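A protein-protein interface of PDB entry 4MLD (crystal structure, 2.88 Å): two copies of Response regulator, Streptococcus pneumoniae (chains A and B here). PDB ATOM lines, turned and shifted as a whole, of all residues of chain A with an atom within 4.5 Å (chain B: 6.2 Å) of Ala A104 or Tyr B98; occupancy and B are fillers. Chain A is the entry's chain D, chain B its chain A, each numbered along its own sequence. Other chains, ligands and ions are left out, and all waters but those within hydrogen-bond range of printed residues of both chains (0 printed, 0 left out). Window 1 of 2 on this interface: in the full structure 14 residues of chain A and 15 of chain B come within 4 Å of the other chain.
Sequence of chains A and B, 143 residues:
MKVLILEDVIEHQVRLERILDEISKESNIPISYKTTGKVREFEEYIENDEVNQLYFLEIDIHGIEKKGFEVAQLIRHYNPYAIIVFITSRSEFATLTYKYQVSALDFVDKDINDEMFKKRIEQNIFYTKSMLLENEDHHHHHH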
ATOM      1  N   ILE A  84       7.520  -6.303 -19.489  1.00  0.00           N
ATOM      2  CA  ILE A  84       7.113  -7.585 -18.934  1.00  0.00           C
ATOM      3  C   ILE A  84       8.237  -8.210 -18.118  1.00  0.00           C
ATOM      4  O   ILE A  84       9.297  -8.527 -18.651  1.00  0.00           O
ATOM      5  CB  ILE A  84       6.702  -8.563 -20.053  1.00  0.00           C
ATOM      6  CG1 ILE A  84       5.669  -7.914 -20.976  1.00  0.00           C
ATOM      7  CG2 ILE A  84       6.173  -9.860 -19.464  1.00  0.00           C
ATOM      8  CD1 ILE A  84       5.253  -8.783 -22.143  1.00  0.00           C
ATOM      9  N   PHE A  86       9.041 -11.383 -15.304  1.00  0.00           N
ATOM     10  CA  PHE A  86       8.520 -12.602 -14.707  1.00  0.00           C
ATOM     11  C   PHE A  86       8.998 -12.753 -13.273  1.00  0.00           C
ATOM     12  O   PHE A  86      10.146 -12.444 -12.953  1.00  0.00           O
ATOM     13  CB  PHE A  86       8.927 -13.828 -15.524  1.00  0.00           C
ATOM     14  CG  PHE A  86       8.338 -13.862 -16.904  1.00  0.00           C
ATOM     15  CD1 PHE A  86       7.064 -14.365 -17.116  1.00  0.00           C
ATOM     16  CD2 PHE A  86       9.057 -13.396 -17.989  1.00  0.00           C
ATOM     17  CE1 PHE A  86       6.518 -14.401 -18.386  1.00  0.00           C
ATOM     18  CE2 PHE A  86       8.517 -13.430 -19.262  1.00  0.00           C
ATOM     19  CZ  PHE A  86       7.246 -13.932 -19.461  1.00  0.00           C
ATOM     20  N   ALA A  94      13.956 -19.582 -17.161  1.00  0.00           N
ATOM     21  CA  ALA A  94      14.648 -18.324 -17.424  1.00  0.00           C
ATOM     22  C   ALA A  94      15.168 -18.229 -18.856  1.00  0.00           C
ATOM     23  O   ALA A  94      15.243 -17.141 -19.428  1.00  0.00           O
ATOM     24  CB  ALA A  94      15.782 -18.126 -16.433  1.00  0.00           C
ATOM     25  N   THR A  97      12.069 -18.049 -22.044  1.00  0.00           N
ATOM     26  CA  THR A  97      11.288 -16.848 -22.343  1.00  0.00           C
ATOM     27  C   THR A  97      11.426 -16.375 -23.788  1.00  0.00           C
ATOM     28  O   THR A  97      10.508 -15.765 -24.338  1.00  0.00           O
ATOM     29  CB  THR A  97      11.660 -15.681 -21.412  1.00  0.00           C
ATOM     30  OG1 THR A  97      12.917 -15.123 -21.816  1.00  0.00           O
ATOM     31  CG2 THR A  97      11.751 -16.155 -19.971  1.00  0.00           C
ATOM     32  N   TYR A  98      12.571 -16.666 -24.395  1.00  0.00           N
ATOM     33  CA  TYR A  98      12.849 -16.246 -25.764  1.00  0.00           C
ATOM     34  C   TYR A  98      11.961 -16.951 -26.789  1.00  0.00           C
ATOM     35  O   TYR A  98      11.564 -16.352 -27.791  1.00  0.00           O
ATOM     36  CB  TYR A  98      14.320 -16.490 -26.106  1.00  0.00           C
ATOM     37  CG  TYR A  98      15.293 -15.844 -25.150  1.00  0.00           C
ATOM     38  CD1 TYR A  98      15.399 -14.462 -25.067  1.00  0.00           C
ATOM     39  CD2 TYR A  98      16.114 -16.616 -24.339  1.00  0.00           C
ATOM     40  CE1 TYR A  98      16.291 -13.866 -24.195  1.00  0.00           C
ATOM     41  CE2 TYR A  98      17.011 -16.030 -23.467  1.00  0.00           C
ATOM     42  CZ  TYR A  98      17.094 -14.654 -23.398  1.00  0.00           C
ATOM     43  OH  TYR A  98      17.985 -14.068 -22.530  1.00  0.00           O
ATOM     44  N   VAL A 102       8.402 -13.046 -26.357  1.00  0.00           N
ATOM     45  CA  VAL A 102       8.218 -11.899 -25.482  1.00  0.00           C
ATOM     46  C   VAL A 102       9.590 -11.255 -25.335  1.00  0.00           C
ATOM     47  O   VAL A 102      10.614 -11.913 -25.524  1.00  0.00           O
ATOM     48  CB  VAL A 102       7.633 -12.294 -24.106  1.00  0.00           C
ATOM     49  CG1 VAL A 102       6.242 -12.883 -24.275  1.00  0.00           C
ATOM     50  CG2 VAL A 102       8.531 -13.298 -23.405  1.00  0.00           C
ATOM     51  N   SER A 103       9.618  -9.962 -25.049  1.00  0.00           N
ATOM     52  CA  SER A 103      10.879  -9.290 -24.781  1.00  0.00           C
ATOM     53  C   SER A 103      10.921  -8.922 -23.313  1.00  0.00           C
ATOM     54  O   SER A 103      10.890  -7.743 -22.957  1.00  0.00           O
ATOM     55  CB  SER A 103      11.045  -8.052 -25.656  1.00  0.00           C
ATOM     56  OG  SER A 103      11.088  -8.415 -27.023  1.00  0.00           O
ATOM     57  N   ALA A 104      10.976  -9.950 -22.470  1.00  0.00           N
ATOM     58  CA  ALA A 104      10.949  -9.770 -21.029  1.00  0.00           C
ATOM     59  C   ALA A 104      12.129  -8.937 -20.560  1.00  0.00           C
ATOM     60  O   ALA A 104      13.278  -9.239 -20.884  1.00  0.00           O
ATOM     61  CB  ALA A 104      10.942 -11.114 -20.332  1.00  0.00           C
ATOM     62  N   LEU A 105      11.839  -7.900 -19.782  1.00  0.00           N
ATOM     63  CA  LEU A 105      12.888  -7.079 -19.202  1.00  0.00           C
ATOM     64  C   LEU A 105      13.696  -7.910 -18.220  1.00  0.00           C
ATOM     65  O   LEU A 105      14.923  -7.985 -18.312  1.00  0.00           O
ATOM     66  CB  LEU A 105      12.295  -5.866 -18.490  1.00  0.00           C
ATOM     67  CG  LEU A 105      13.318  -5.004 -17.753  1.00  0.00           C
ATOM     68  CD1 LEU A 105      14.216  -4.275 -18.742  1.00  0.00           C
ATOM     69  CD2 LEU A 105      12.627  -4.026 -16.816  1.00  0.00           C
ATOM     70  N   ASP A 106      12.996  -8.543 -17.286  1.00  0.00           N
ATOM     71  CA  ASP A 106      13.656  -9.276 -16.220  1.00  0.00           C
ATOM     72  C   ASP A 106      12.968 -10.604 -15.913  1.00  0.00           C
ATOM     73  O   ASP A 106      11.838 -10.851 -16.335  1.00  0.00           O
ATOM     74  CB  ASP A 106      13.701  -8.418 -14.956  1.00  0.00           C
ATOM     75  CG  ASP A 106      14.888  -8.740 -14.073  1.00  0.00           C
ATOM     76  OD1 ASP A 106      15.569  -9.753 -14.331  1.00  0.00           O
ATOM     77  OD2 ASP A 106      15.135  -7.981 -13.111  1.00  0.00           O
ATOM     78  N   PHE A 107      13.669 -11.449 -15.166  1.00  0.00           N
ATOM     79  CA  PHE A 107      13.158 -12.746 -14.749  1.00  0.00           C
ATOM     80  C   PHE A 107      13.567 -12.950 -13.297  1.00  0.00           C
ATOM     81  O   PHE A 107      14.705 -13.321 -13.014  1.00  0.00           O
ATOM     82  CB  PHE A 107      13.753 -13.844 -15.630  1.00  0.00           C
ATOM     83  CG  PHE A 107      13.156 -15.206 -15.403  1.00  0.00           C
ATOM     84  CD1 PHE A 107      12.114 -15.660 -16.196  1.00  0.00           C
ATOM     85  CD2 PHE A 107      13.648 -16.038 -14.410  1.00  0.00           C
ATOM     86  CE1 PHE A 107      11.567 -16.911 -15.997  1.00  0.00           C
ATOM     87  CE2 PHE A 107      13.105 -17.291 -14.207  1.00  0.00           C
ATOM     88  CZ  PHE A 107      12.065 -17.728 -15.005  1.00  0.00           C
ATOM     89  N   ALA B  94      23.075 -16.702 -21.390  1.00  0.00           N
ATOM     90  CA  ALA B  94      21.649 -16.679 -21.721  1.00  0.00           C
ATOM     91  C   ALA B  94      20.789 -16.077 -20.613  1.00  0.00           C
ATOM     92  O   ALA B  94      19.831 -15.353 -20.881  1.00  0.00           O
ATOM     93  CB  ALA B  94      21.165 -18.077 -22.063  1.00  0.00           C
ATOM     94  N   THR B  95      21.142 -16.379 -19.369  1.00  0.00           N
ATOM     95  CA  THR B  95      20.393 -15.891 -18.219  1.00  0.00           C
ATOM     96  C   THR B  95      20.932 -14.566 -17.683  1.00  0.00           C
ATOM     97  O   THR B  95      20.401 -14.023 -16.716  1.00  0.00           O
ATOM     98  CB  THR B  95      20.386 -16.925 -17.080  1.00  0.00           C
ATOM     99  OG1 THR B  95      21.716 -17.420 -16.875  1.00  0.00           O
ATOM    100  CG2 THR B  95      19.472 -18.089 -17.427  1.00  0.00           C
ATOM    101  N   LEU B  96      21.980 -14.045 -18.314  1.00  0.00           N
ATOM    102  CA  LEU B  96      22.606 -12.805 -17.860  1.00  0.00           C
ATOM    103  C   LEU B  96      22.109 -11.577 -18.615  1.00  0.00           C
ATOM    104  O   LEU B  96      22.467 -10.449 -18.277  1.00  0.00           O
ATOM    105  CB  LEU B  96      24.127 -12.898 -17.979  1.00  0.00           C
ATOM    106  CG  LEU B  96      24.828 -13.936 -17.103  1.00  0.00           C
ATOM    107  CD1 LEU B  96      26.321 -13.926 -17.375  1.00  0.00           C
ATOM    108  CD2 LEU B  96      24.547 -13.676 -15.632  1.00  0.00           C
ATOM    109  N   THR B  97      21.288 -11.796 -19.637  1.00  0.00           N
ATOM    110  CA  THR B  97      20.760 -10.697 -20.439  1.00  0.00           C
ATOM    111  C   THR B  97      19.871  -9.776 -19.606  1.00  0.00           C
ATOM    112  O   THR B  97      19.828  -8.566 -19.834  1.00  0.00           O
ATOM    113  CB  THR B  97      19.946 -11.215 -21.642  1.00  0.00           C
ATOM    114  OG1 THR B  97      18.741 -11.838 -21.178  1.00  0.00           O
ATOM    115  CG2 THR B  97      20.760 -12.217 -22.450  1.00  0.00           C
ATOM    116  N   TYR B  98      19.174 -10.357 -18.633  1.00  0.00           N
ATOM    117  CA  TYR B  98      18.207  -9.621 -17.826  1.00  0.00           C
ATOM    118  C   TYR B  98      18.873  -8.600 -16.903  1.00  0.00           C
ATOM    119  O   TYR B  98      18.263  -7.594 -16.535  1.00  0.00           O
ATOM    120  CB  TYR B  98      17.355 -10.588 -16.997  1.00  0.00           C
ATOM    121  CG  TYR B  98      16.681 -11.682 -17.798  1.00  0.00           C
ATOM    122  CD1 TYR B  98      15.646 -11.390 -18.677  1.00  0.00           C
ATOM    123  CD2 TYR B  98      17.068 -13.010 -17.661  1.00  0.00           C
ATOM    124  CE1 TYR B  98      15.025 -12.387 -19.410  1.00  0.00           C
ATOM    125  CE2 TYR B  98      16.452 -14.016 -18.387  1.00  0.00           C
ATOM    126  CZ  TYR B  98      15.431 -13.698 -19.260  1.00  0.00           C
ATOM    127  OH  TYR B  98      14.816 -14.694 -19.983  1.00  0.00           O
ATOM    128  N   LYS B  99      20.120  -8.869 -16.527  1.00  0.00           N
ATOM    129  CA  LYS B  99      20.866  -7.984 -15.636  1.00  0.00           C
ATOM    130  C   LYS B  99      21.115  -6.618 -16.263  1.00  0.00           C
ATOM    131  O   LYS B  99      21.120  -5.601 -15.571  1.00  0.00           O
ATOM    132  CB  LYS B  99      22.203  -8.616 -15.252  1.00  0.00           C
ATOM    133  CG  LYS B  99      22.087  -9.909 -14.470  1.00  0.00           C
ATOM    134  CD  LYS B  99      23.461 -10.513 -14.245  1.00  0.00           C
ATOM    135  CE  LYS B  99      23.836 -10.541 -12.774  1.00  0.00           C
ATOM    136  NZ  LYS B  99      23.342 -11.773 -12.099  1.00  0.00           N
ATOM    137  N   TYR B 100      21.322  -6.599 -17.575  1.00  0.00           N
ATOM    138  CA  TYR B 100      21.631  -5.360 -18.281  1.00  0.00           C
ATOM    139  C   TYR B 100      20.378  -4.596 -18.696  1.00  0.00           C
ATOM    140  O   TYR B 100      20.462  -3.557 -19.353  1.00  0.00           O
ATOM    141  CB  TYR B 100      22.529  -5.645 -19.485  1.00  0.00           C
ATOM    142  CG  TYR B 100      23.893  -6.150 -19.077  1.00  0.00           C
ATOM    143  CD1 TYR B 100      24.962  -5.275 -18.931  1.00  0.00           C
ATOM    144  CD2 TYR B 100      24.104  -7.495 -18.807  1.00  0.00           C
ATOM    145  CE1 TYR B 100      26.206  -5.728 -18.545  1.00  0.00           C
ATOM    146  CE2 TYR B 100      25.343  -7.958 -18.419  1.00  0.00           C
ATOM    147  CZ  TYR B 100      26.390  -7.071 -18.290  1.00  0.00           C
ATOM    148  OH  TYR B 100      27.628  -7.532 -17.906  1.00  0.00           O
ATOM    149  N   GLN B 101      19.222  -5.121 -18.299  1.00  0.00           N
ATOM    150  CA  GLN B 101      17.927  -4.489 -18.552  1.00  0.00           C
ATOM    151  C   GLN B 101      17.659  -4.186 -20.023  1.00  0.00           C
ATOM    152  O   GLN B 101      16.888  -3.288 -20.360  1.00  0.00           O
ATOM    153  CB  GLN B 101      17.746  -3.240 -17.690  1.00  0.00           C
ATOM    154  CG  GLN B 101      17.549  -3.555 -16.218  1.00  0.00           C
ATOM    155  CD  GLN B 101      17.440  -2.314 -15.366  1.00  0.00           C
ATOM    156  OE1 GLN B 101      17.921  -1.244 -15.740  1.00  0.00           O
ATOM    157  NE2 GLN B 101      16.801  -2.448 -14.210  1.00  0.00           N
ATOM    158  N   VAL B 102      18.309  -4.942 -20.895  1.00  0.00           N
ATOM    159  CA  VAL B 102      17.934  -4.967 -22.291  1.00  0.00           C
ATOM    160  C   VAL B 102      16.747  -5.915 -22.379  1.00  0.00           C
ATOM    161  O   VAL B 102      16.524  -6.725 -21.476  1.00  0.00           O
ATOM    162  CB  VAL B 102      19.089  -5.471 -23.164  1.00  0.00           C
ATOM    163  CG1 VAL B 102      20.275  -4.531 -23.039  1.00  0.00           C
ATOM    164  CG2 VAL B 102      19.488  -6.881 -22.759  1.00  0.00           C
ATOM    165  N   SER B 103      15.966  -5.803 -23.443  1.00  0.00           N
ATOM    166  CA  SER B 103      14.818  -6.682 -23.604  1.00  0.00           C
ATOM    167  C   SER B 103      14.990  -7.483 -24.880  1.00  0.00           C
ATOM    168  O   SER B 103      14.298  -7.259 -25.873  1.00  0.00           O
ATOM    169  CB  SER B 103      13.517  -5.881 -23.612  1.00  0.00           C
ATOM    170  OG  SER B 103      13.341  -5.204 -22.376  1.00  0.00           O
ATOM    171  N   ALA B 104      15.937  -8.413 -24.838  1.00  0.00           N
ATOM    172  CA  ALA B 104      16.319  -9.184 -26.009  1.00  0.00           C
ATOM    173  C   ALA B 104      15.171 -10.048 -26.508  1.00  0.00           C
ATOM    174  O   ALA B 104      14.517 -10.738 -25.726  1.00  0.00           O
ATOM    175  CB  ALA B 104      17.537 -10.041 -25.699  1.00  0.00           C
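Ala A94 touches Tyr B98, and with the chains exchanged Tyr A98 touches Ala B94. Thr A97 touches Tyr B98, and with the chains exchanged Tyr A98 touches Thr B97. Tyr A98 touches Ala B104, and with the chains exchanged Ala A104 touches Tyr B98. Ser B103 touches its own counterpart, Ser A103. 6 positions are printed for both chains.
Tyr B98 touches just these residues of chain A: Ala A94 (2.5 Å), Thr A97 (2.7 Å), Ala A104 (3.9 Å), Leu A105 (3.5 Å), Asp A106 (3.3 Å) and Phe A107 (3.9 Å). Of the printed residues of chain B, Ser A103 touches Ser B103. Of the printed residues of chain A, Thr B97 touches Tyr A98 (2.7 Å). Of the printed residues of chain A, Ala B94 touches Tyr A98. Printed residues of chain A within 4 Å of Val B102: Leu A105 (3.8 Å). Tyr B100 touches none of the printed residues of chain A. The nearest printed residue of chain B that does not touch Asp A106 is Lys B99 (5.1 Å).
O of Ala B94 sits at hydrogen-bond distance from OH of Tyr A98 (2.8 Å). The side-chain hydroxyl (OG1) of Thr B97 is in hydrogen-bond range of the side-chain hydroxyl (OH) of Tyr A98 (2.7 Å). OH of Tyr B98 lies within hydrogen-bond range of O of Ala A94 (2.5 Å). OH of Tyr B98 is in hydrogen-bond range of OG1 of Thr A97 (2.7 Å).
Hydrophobic or aromatic side chains of chain A within 4 Å of the printed part of chain B: Ala A94, Tyr A98, Leu A105 and Phe A107. Among the printed residues, no Asp or Glu carboxylate lies within 4 Å of a Lys or Arg side-chain nitrogen of the other chain.
N of Leu A105 sits at hydrogen-bond distance from O of Ile A84 (2.9 Å). The backbone carbonyl oxygen (O) of Asp A106 sits at hydrogen-bond distance from the backbone NH (N) of Phe A86, 3.0 Å away.
Thr B95 touches Ala A94 (CG2 to CB, 3.8 Å). Ala B104 touches Tyr A98. Ser A103 touches Ser B103. Ala A104 touches Tyr B98 (O to CD1, 3.9 Å). Tyr B98 touches Leu A105. Leu A105 touches Gln B101. Leu A105 touches Val B102 (O to O, 3.8 Å). Ser B103 touches Leu A105. Asp A106 touches Tyr B98. Phe A107 touches Tyr B98 (CB to CE2, 3.9 Å).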
